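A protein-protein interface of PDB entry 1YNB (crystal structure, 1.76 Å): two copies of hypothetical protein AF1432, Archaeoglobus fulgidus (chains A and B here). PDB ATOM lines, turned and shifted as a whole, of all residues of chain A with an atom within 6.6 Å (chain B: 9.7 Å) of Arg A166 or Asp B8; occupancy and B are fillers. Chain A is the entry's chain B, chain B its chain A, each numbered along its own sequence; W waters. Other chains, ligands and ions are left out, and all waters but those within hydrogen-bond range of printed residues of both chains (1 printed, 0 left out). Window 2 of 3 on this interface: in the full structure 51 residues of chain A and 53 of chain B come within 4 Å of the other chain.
The guanidinium group (NE) of Arg A166 is in salt-bridge range of the side-chain carboxylate (OD2) of Asp B8 (3.8 Å).
The side-chain amino group (NZ) of Lys B12 lies close to the guanidinium group (NH1) of Arg A166 (2.5 Å).
The backbone carbonyl oxygen (O) of Asn A168 is in hydrogen-bond range of the guanidinium group (NH2) of Arg A166 (3.1 Å).
N of Val A170 sits at hydrogen-bond distance from OD1 of Asn A168 (3.2 Å).
Among the printed residues, pairs that only touch across the chains: Asn A168 with His B15 (3.5 Å), Trp A171 with Lys B12 (3.5 Å), Trp A171 with Glu B16 (3.5 Å), Val A162 with Asp B8 (3.6 Å), Leu A163 with His B15 (3.6 Å), Val A170 with Lys B12 (3.7 Å), Trp A171 with His B15 (3.7 Å), Arg A166 with Val B11 (3.7 Å), Asn A168 with Lys B12 (3.7 Å), Val A162 with Val B11 (3.8 Å), Pro A169 with His B15 (3.8 Å), Val A162 with Met B7 (3.9 Å) and Leu A163 with Val B11 (3.9 Å).
Of chain B, only Asp B8, Val B11 and Lys B12 come within 4 Å of Arg A166.
Of the printed residues of chain A, Asp B8 touches Val A162 and Arg A166.
Asn A168 touches just these residues of chain B: Lys B12 and His B15.
Printed residues of chain B within 4 Å of Val A170: Lys B12 (3.7 Å).
Of the printed residues of chain A, Val B11 touches Val A162, Leu A163 and Arg A166.
Printed residues of chain B within 4 Å of Trp A171: Lys B12, His B15 and Glu B16.
The nearest residue of chain B that does not touch Arg A166 is His B15 (4.04 Å).
Printed residues of chain B that touch a printed residue of chain A: Met B7, Asp B8, Val B11, Lys B12, His B15 and Glu B16.
Along chain A the printed residues that touch a printed residue of chain B span positions 162 to 171.
Among the printed residues, Asp or Glu carboxylates within 4 Å of a Lys or Arg side-chain nitrogen of the other chain: Arg A166 with Asp B8 (3.8 Å).
No position is printed for both chains.
Of the 15 pairs that touch across the chains among the printed residues, none has its exchanged pair printed and touching as well.
Water W1 lies within hydrogen-bond range of NE2 of His B15 (2.9 Å), N of Asn A168 (2.9 Å), O of Leu A163 (3.1 Å) and N of Lys A167 (3.3 Å).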
ATOM      1  N   VAL A 133     -28.610 -12.104   1.781  1.00  0.00           N
ATOM      2  CA  VAL A 133     -28.049 -11.259   2.834  1.00  0.00           C
ATOM      3  C   VAL A 133     -26.751 -10.632   2.326  1.00  0.00           C
ATOM      4  O   VAL A 133     -26.524  -9.453   2.571  1.00  0.00           O
ATOM      5  CB  VAL A 133     -27.755 -12.064   4.099  1.00  0.00           C
ATOM      6  CG1 VAL A 133     -26.906 -11.284   5.085  1.00  0.00           C
ATOM      7  CG2 VAL A 133     -29.094 -12.376   4.772  1.00  0.00           C
ATOM      8  N   ARG A 161     -32.219 -18.929  11.244  1.00  0.00           N
ATOM      9  CA  ARG A 161     -32.538 -17.989  12.309  1.00  0.00           C
ATOM     10  C   ARG A 161     -31.332 -17.144  12.684  1.00  0.00           C
ATOM     11  O   ARG A 161     -31.449 -15.935  12.859  1.00  0.00           O
ATOM     12  CB  ARG A 161     -33.060 -18.729  13.567  1.00  0.00           C
ATOM     13  CG  ARG A 161     -33.452 -17.749  14.689  1.00  0.00           C
ATOM     14  CD  ARG A 161     -34.086 -18.395  15.934  1.00  0.00           C
ATOM     15  NE  ARG A 161     -34.500 -17.363  16.898  1.00  0.00           N
ATOM     16  CZ  ARG A 161     -34.783 -17.606  18.181  1.00  0.00           C
ATOM     17  NH1 ARG A 161     -34.699 -18.842  18.651  1.00  0.00           N
ATOM     18  NH2 ARG A 161     -35.153 -16.627  18.994  1.00  0.00           N
ATOM     19  N   VAL A 162     -30.166 -17.779  12.833  1.00  0.00           N
ATOM     20  CA  VAL A 162     -28.962 -17.034  13.192  1.00  0.00           C
ATOM     21  C   VAL A 162     -28.525 -16.162  11.998  1.00  0.00           C
ATOM     22  O   VAL A 162     -28.104 -15.013  12.197  1.00  0.00           O
ATOM     23  CB  VAL A 162     -27.802 -17.975  13.646  1.00  0.00           C
ATOM     24  CG1 VAL A 162     -26.522 -17.186  13.868  1.00  0.00           C
ATOM     25  CG2 VAL A 162     -28.204 -18.661  14.982  1.00  0.00           C
ATOM     26  N   LEU A 163     -28.646 -16.691  10.784  1.00  0.00           N
ATOM     27  CA  LEU A 163     -28.299 -15.902   9.587  1.00  0.00           C
ATOM     28  C   LEU A 163     -29.032 -14.564   9.629  1.00  0.00           C
ATOM     29  O   LEU A 163     -28.419 -13.509   9.413  1.00  0.00           O
ATOM     30  CB  LEU A 163     -28.714 -16.622   8.311  1.00  0.00           C
ATOM     31  CG  LEU A 163     -28.670 -15.804   6.995  1.00  0.00           C
ATOM     32  CD1 LEU A 163     -27.221 -15.494   6.579  1.00  0.00           C
ATOM     33  CD2 LEU A 163     -29.418 -16.541   5.887  1.00  0.00           C
ATOM     34  N   MET A 164     -30.338 -14.614   9.876  1.00  0.00           N
ATOM     35  CA  MET A 164     -31.170 -13.411   9.882  1.00  0.00           C
ATOM     36  C   MET A 164     -31.071 -12.554  11.131  1.00  0.00           C
ATOM     37  O   MET A 164     -31.348 -11.346  11.098  1.00  0.00           O
ATOM     38  CB  MET A 164     -32.627 -13.786   9.595  1.00  0.00           C
ATOM     39  CG  MET A 164     -32.851 -14.541   8.242  1.00  0.00           C
ATOM     40  SD  MET A 164     -32.265 -13.564   6.799  1.00  0.00           S
ATOM     41  CE  MET A 164     -33.718 -12.474   6.551  1.00  0.00           C
ATOM     42  N   GLU A 165     -30.678 -13.170  12.234  1.00  0.00           N
ATOM     43  CA  GLU A 165     -30.505 -12.454  13.489  1.00  0.00           C
ATOM     44  C   GLU A 165     -29.241 -11.608  13.346  1.00  0.00           C
ATOM     45  O   GLU A 165     -29.168 -10.470  13.802  1.00  0.00           O
ATOM     46  CB  GLU A 165     -30.389 -13.512  14.587  1.00  0.00           C
ATOM     47  CG  GLU A 165     -29.739 -13.170  15.889  1.00  0.00           C
ATOM     48  CD  GLU A 165     -29.918 -14.328  16.874  1.00  0.00           C
ATOM     49  OE1 GLU A 165     -29.911 -15.511  16.429  1.00  0.00           O
ATOM     50  OE2 GLU A 165     -30.066 -14.052  18.082  1.00  0.00           O
ATOM     51  N   ARG A 166     -28.265 -12.147  12.634  1.00  0.00           N
ATOM     52  CA  ARG A 166     -27.005 -11.462  12.486  1.00  0.00           C
ATOM     53  C   ARG A 166     -26.890 -10.549  11.268  1.00  0.00           C
ATOM     54  O   ARG A 166     -26.296  -9.478  11.388  1.00  0.00           O
ATOM     55  CB  ARG A 166     -25.883 -12.497  12.457  1.00  0.00           C
ATOM     56  CG  ARG A 166     -25.587 -13.124  13.825  1.00  0.00           C
ATOM     57  CD  ARG A 166     -24.764 -14.401  13.693  1.00  0.00           C
ATOM     58  NE  ARG A 166     -24.032 -14.391  12.437  1.00  0.00           N
ATOM     59  CZ  ARG A 166     -22.878 -13.765  12.225  1.00  0.00           C
ATOM     60  NH1 ARG A 166     -22.270 -13.103  13.211  1.00  0.00           N
ATOM     61  NH2 ARG A 166     -22.385 -13.731  10.993  1.00  0.00           N
ATOM     62  N   LYS A 167     -27.478 -10.965  10.136  1.00  0.00           N
ATOM     63  CA  LYS A 167     -27.395 -10.244   8.858  1.00  0.00           C
ATOM     64  C   LYS A 167     -26.040  -9.567   8.754  1.00  0.00           C
ATOM     65  O   LYS A 167     -25.919  -8.370   8.553  1.00  0.00           O
ATOM     66  CB  LYS A 167     -28.523  -9.221   8.713  1.00  0.00           C
ATOM     67  CG  LYS A 167     -29.884  -9.853   8.529  1.00  0.00           C
ATOM     68  CD  LYS A 167     -30.915  -8.810   8.056  1.00  0.00           C
ATOM     69  CE  LYS A 167     -32.335  -9.369   8.030  1.00  0.00           C
ATOM     70  NZ  LYS A 167     -32.922  -9.480   9.387  1.00  0.00           N
ATOM     71  N   ASN A 168     -25.004 -10.366   8.917  1.00  0.00           N
ATOM     72  CA  ASN A 168     -23.654  -9.858   8.869  1.00  0.00           C
ATOM     73  C   ASN A 168     -22.729 -10.777   8.078  1.00  0.00           C
ATOM     74  O   ASN A 168     -22.165 -11.738   8.614  1.00  0.00           O
ATOM     75  CB  ASN A 168     -23.143  -9.678  10.292  1.00  0.00           C
ATOM     76  CG  ASN A 168     -21.725  -9.200  10.334  1.00  0.00           C
ATOM     77  OD1 ASN A 168     -21.210  -8.661   9.349  1.00  0.00           O
ATOM     78  ND2 ASN A 168     -21.073  -9.389  11.481  1.00  0.00           N
ATOM     79  N   PRO A 169     -22.525 -10.468   6.792  1.00  0.00           N
ATOM     80  CA  PRO A 169     -21.666 -11.272   5.919  1.00  0.00           C
ATOM     81  C   PRO A 169     -20.158 -11.176   6.155  1.00  0.00           C
ATOM     82  O   PRO A 169     -19.371 -11.905   5.549  1.00  0.00           O
ATOM     83  CB  PRO A 169     -22.100 -10.838   4.514  1.00  0.00           C
ATOM     84  CG  PRO A 169     -22.542  -9.434   4.692  1.00  0.00           C
ATOM     85  CD  PRO A 169     -23.225  -9.403   6.047  1.00  0.00           C
ATOM     86  N   VAL A 170     -19.763 -10.297   7.063  1.00  0.00           N
ATOM     87  CA  VAL A 170     -18.358 -10.130   7.362  1.00  0.00           C
ATOM     88  C   VAL A 170     -17.922 -11.275   8.234  1.00  0.00           C
ATOM     89  O   VAL A 170     -18.180 -11.288   9.441  1.00  0.00           O
ATOM     90  CB  VAL A 170     -18.106  -8.835   8.104  1.00  0.00           C
ATOM     91  CG1 VAL A 170     -16.644  -8.687   8.365  1.00  0.00           C
ATOM     92  CG2 VAL A 170     -18.661  -7.683   7.304  1.00  0.00           C
ATOM     93  N   TRP A 171     -17.232 -12.219   7.630  1.00  0.00           N
ATOM     94  CA  TRP A 171     -16.807 -13.399   8.347  1.00  0.00           C
ATOM     95  C   TRP A 171     -15.396 -13.297   8.826  1.00  0.00           C
ATOM     96  O   TRP A 171     -14.952 -14.110   9.609  1.00  0.00           O
ATOM     97  CB  TRP A 171     -16.941 -14.619   7.445  1.00  0.00           C
ATOM     98  CG  TRP A 171     -16.251 -14.439   6.094  1.00  0.00           C
ATOM     99  CD1 TRP A 171     -16.822 -14.022   4.904  1.00  0.00           C
ATOM    100  CD2 TRP A 171     -14.893 -14.713   5.813  1.00  0.00           C
ATOM    101  NE1 TRP A 171     -15.879 -14.039   3.894  1.00  0.00           N
ATOM    102  CE2 TRP A 171     -14.684 -14.457   4.429  1.00  0.00           C
ATOM    103  CE3 TRP A 171     -13.810 -15.158   6.597  1.00  0.00           C
ATOM    104  CZ2 TRP A 171     -13.434 -14.635   3.816  1.00  0.00           C
ATOM    105  CZ3 TRP A 171     -12.565 -15.338   5.973  1.00  0.00           C
ATOM    106  CH2 TRP A 171     -12.394 -15.078   4.606  1.00  0.00           C
ATOM    107  N   MET B   7     -24.088 -21.885  16.766  1.00  0.00           N
ATOM    108  CA  MET B   7     -24.495 -21.902  15.332  1.00  0.00           C
ATOM    109  C   MET B   7     -23.910 -20.663  14.646  1.00  0.00           C
ATOM    110  O   MET B   7     -23.929 -20.554  13.424  1.00  0.00           O
ATOM    111  CB  MET B   7     -26.020 -21.896  15.227  1.00  0.00           C
ATOM    112  CG  MET B   7     -26.588 -22.630  14.012  1.00  0.00           C
ATOM    113  SD  MET B   7     -26.119 -24.401  13.976  1.00  0.00           S
ATOM    114  CE  MET B   7     -26.940 -24.977  15.535  1.00  0.00           C
ATOM    115  N   ASP B   8     -23.388 -19.734  15.438  1.00  0.00           N
ATOM    116  CA  ASP B   8     -22.788 -18.522  14.875  1.00  0.00           C
ATOM    117  C   ASP B   8     -21.522 -18.828  14.094  1.00  0.00           C
ATOM    118  O   ASP B   8     -21.229 -18.175  13.086  1.00  0.00           O
ATOM    119  CB  ASP B   8     -22.475 -17.519  15.980  1.00  0.00           C
ATOM    120  CG  ASP B   8     -23.724 -16.835  16.492  1.00  0.00           C
ATOM    121  OD1 ASP B   8     -24.410 -17.425  17.368  1.00  0.00           O
ATOM    122  OD2 ASP B   8     -24.029 -15.723  15.994  1.00  0.00           O
ATOM    123  N   ASP B   9     -20.754 -19.803  14.582  1.00  0.00           N
ATOM    124  CA  ASP B   9     -19.535 -20.200  13.897  1.00  0.00           C
ATOM    125  C   ASP B   9     -19.904 -20.832  12.569  1.00  0.00           C
ATOM    126  O   ASP B   9     -19.216 -20.646  11.578  1.00  0.00           O
ATOM    127  CB  ASP B   9     -18.749 -21.210  14.731  1.00  0.00           C
ATOM    128  CG  ASP B   9     -17.940 -20.547  15.811  1.00  0.00           C
ATOM    129  OD1 ASP B   9     -18.421 -19.521  16.355  1.00  0.00           O
ATOM    130  OD2 ASP B   9     -16.826 -21.054  16.127  1.00  0.00           O
ATOM    131  N   VAL B  10     -20.994 -21.575  12.545  1.00  0.00           N
ATOM    132  CA  VAL B  10     -21.405 -22.222  11.314  1.00  0.00           C
ATOM    133  C   VAL B  10     -21.885 -21.170  10.322  1.00  0.00           C
ATOM    134  O   VAL B  10     -21.568 -21.230   9.130  1.00  0.00           O
ATOM    135  CB  VAL B  10     -22.526 -23.247  11.580  1.00  0.00           C
ATOM    136  CG1 VAL B  10     -23.121 -23.732  10.260  1.00  0.00           C
ATOM    137  CG2 VAL B  10     -21.944 -24.445  12.368  1.00  0.00           C
ATOM    138  N   VAL B  11     -22.648 -20.202  10.800  1.00  0.00           N
ATOM    139  CA  VAL B  11     -23.132 -19.182   9.878  1.00  0.00           C
ATOM    140  C   VAL B  11     -21.920 -18.414   9.317  1.00  0.00           C
ATOM    141  O   VAL B  11     -21.840 -18.204   8.123  1.00  0.00           O
ATOM    142  CB  VAL B  11     -24.163 -18.249  10.585  1.00  0.00           C
ATOM    143  CG1 VAL B  11     -24.415 -16.962   9.784  1.00  0.00           C
ATOM    144  CG2 VAL B  11     -25.475 -19.020  10.727  1.00  0.00           C
ATOM    145  N   LYS B  12     -20.963 -18.031  10.148  1.00  0.00           N
ATOM    146  CA  LYS B  12     -19.793 -17.327   9.592  1.00  0.00           C
ATOM    147  C   LYS B  12     -19.034 -18.194   8.587  1.00  0.00           C
ATOM    148  O   LYS B  12     -18.521 -17.701   7.567  1.00  0.00           O
ATOM    149  CB  LYS B  12     -18.864 -16.845  10.716  1.00  0.00           C
ATOM    150  CG  LYS B  12     -19.206 -15.425  11.148  1.00  0.00           C
ATOM    151  CD  LYS B  12     -18.365 -14.905  12.291  1.00  0.00           C
ATOM    152  CE  LYS B  12     -18.577 -13.363  12.449  1.00  0.00           C
ATOM    153  NZ  LYS B  12     -20.010 -12.881  12.244  1.00  0.00           N
ATOM    154  N   PHE B  13     -18.914 -19.496   8.875  1.00  0.00           N
ATOM    155  CA  PHE B  13     -18.250 -20.389   7.950  1.00  0.00           C
ATOM    156  C   PHE B  13     -18.991 -20.418   6.598  1.00  0.00           C
ATOM    157  O   PHE B  13     -18.349 -20.420   5.537  1.00  0.00           O
ATOM    158  CB  PHE B  13     -18.170 -21.824   8.537  1.00  0.00           C
ATOM    159  CG  PHE B  13     -17.675 -22.860   7.565  1.00  0.00           C
ATOM    160  CD1 PHE B  13     -16.339 -22.923   7.208  1.00  0.00           C
ATOM    161  CD2 PHE B  13     -18.558 -23.789   6.999  1.00  0.00           C
ATOM    162  CE1 PHE B  13     -15.885 -23.883   6.310  1.00  0.00           C
ATOM    163  CE2 PHE B  13     -18.113 -24.761   6.093  1.00  0.00           C
ATOM    164  CZ  PHE B  13     -16.780 -24.813   5.745  1.00  0.00           C
ATOM    165  N   ILE B  14     -20.324 -20.432   6.611  1.00  0.00           N
ATOM    166  CA  ILE B  14     -21.052 -20.481   5.344  1.00  0.00           C
ATOM    167  C   ILE B  14     -20.807 -19.172   4.552  1.00  0.00           C
ATOM    168  O   ILE B  14     -20.649 -19.227   3.334  1.00  0.00           O
ATOM    169  CB  ILE B  14     -22.562 -20.739   5.564  1.00  0.00           C
ATOM    170  CG1 ILE B  14     -22.719 -22.202   6.075  1.00  0.00           C
ATOM    171  CG2 ILE B  14     -23.337 -20.629   4.223  1.00  0.00           C
ATOM    172  CD1 ILE B  14     -24.103 -22.551   6.718  1.00  0.00           C
ATOM    173  N   HIS B  15     -20.755 -18.046   5.259  1.00  0.00           N
ATOM    174  CA  HIS B  15     -20.470 -16.743   4.618  1.00  0.00           C
ATOM    175  C   HIS B  15     -19.071 -16.833   4.044  1.00  0.00           C
ATOM    176  O   HIS B  15     -18.803 -16.408   2.893  1.00  0.00           O
ATOM    177  CB  HIS B  15     -20.511 -15.590   5.631  1.00  0.00           C
ATOM    178  CG  HIS B  15     -21.892 -15.086   5.933  1.00  0.00           C
ATOM    179  ND1 HIS B  15     -22.806 -14.784   4.946  1.00  0.00           N
ATOM    180  CD2 HIS B  15     -22.515 -14.838   7.107  1.00  0.00           C
ATOM    181  CE1 HIS B  15     -23.933 -14.382   5.499  1.00  0.00           C
ATOM    182  NE2 HIS B  15     -23.785 -14.403   6.811  1.00  0.00           N
ATOM    183  N   GLU B  16     -18.155 -17.408   4.828  1.00  0.00           N
ATOM    184  CA  GLU B  16     -16.761 -17.510   4.374  1.00  0.00           C
ATOM    185  C   GLU B  16     -16.620 -18.367   3.131  1.00  0.00           C
ATOM    186  O   GLU B  16     -15.840 -18.057   2.234  1.00  0.00           O
ATOM    187  CB  GLU B  16     -15.851 -18.069   5.507  1.00  0.00           C
ATOM    188  CG  GLU B  16     -14.407 -18.336   5.030  1.00  0.00           C
ATOM    189  CD  GLU B  16     -13.449 -18.708   6.168  1.00  0.00           C
ATOM    190  OE1 GLU B  16     -13.875 -18.661   7.343  1.00  0.00           O
ATOM    191  OE2 GLU B  16     -12.270 -19.028   5.885  1.00  0.00           O
ATOM    192  N   SER B 105     -12.680 -25.073  12.624  1.00  0.00           N
ATOM    193  CA  SER B 105     -12.810 -25.164  14.085  1.00  0.00           C
ATOM    194  C   SER B 105     -14.239 -25.468  14.544  1.00  0.00           C
ATOM    195  O   SER B 105     -14.448 -26.060  15.603  1.00  0.00           O
ATOM    196  CB  SER B 105     -12.336 -23.864  14.740  1.00  0.00           C
ATOM    197  OG  SER B 105     -13.156 -22.764  14.372  1.00  0.00           O
ATOM    198  N   TRP B 106     -15.222 -25.075  13.746  1.00  0.00           N
ATOM    199  CA  TRP B 106     -16.610 -25.319  14.109  1.00  0.00           C
ATOM    200  C   TRP B 106     -16.968 -26.808  14.082  1.00  0.00           C
ATOM    201  O   TRP B 106     -17.968 -27.218  14.670  1.00  0.00           O
ATOM    202  CB  TRP B 106     -17.557 -24.558  13.170  1.00  0.00           C
ATOM    203  CG  TRP B 106     -17.462 -24.995  11.749  1.00  0.00           C
ATOM    204  CD1 TRP B 106     -16.600 -24.526  10.803  1.00  0.00           C
ATOM    205  CD2 TRP B 106     -18.204 -26.057  11.124  1.00  0.00           C
ATOM    206  NE1 TRP B 106     -16.753 -25.230   9.628  1.00  0.00           N
ATOM    207  CE2 TRP B 106     -17.729 -26.175   9.798  1.00  0.00           C
ATOM    208  CE3 TRP B 106     -19.221 -26.923  11.562  1.00  0.00           C
ATOM    209  CZ2 TRP B 106     -18.231 -27.127   8.901  1.00  0.00           C
ATOM    210  CZ3 TRP B 106     -19.722 -27.874  10.666  1.00  0.00           C
ATOM    211  CH2 TRP B 106     -19.223 -27.967   9.351  1.00  0.00           C
HETATM  212  O   HOH W   1     -25.420 -13.249   8.854  1.00  0.00           O
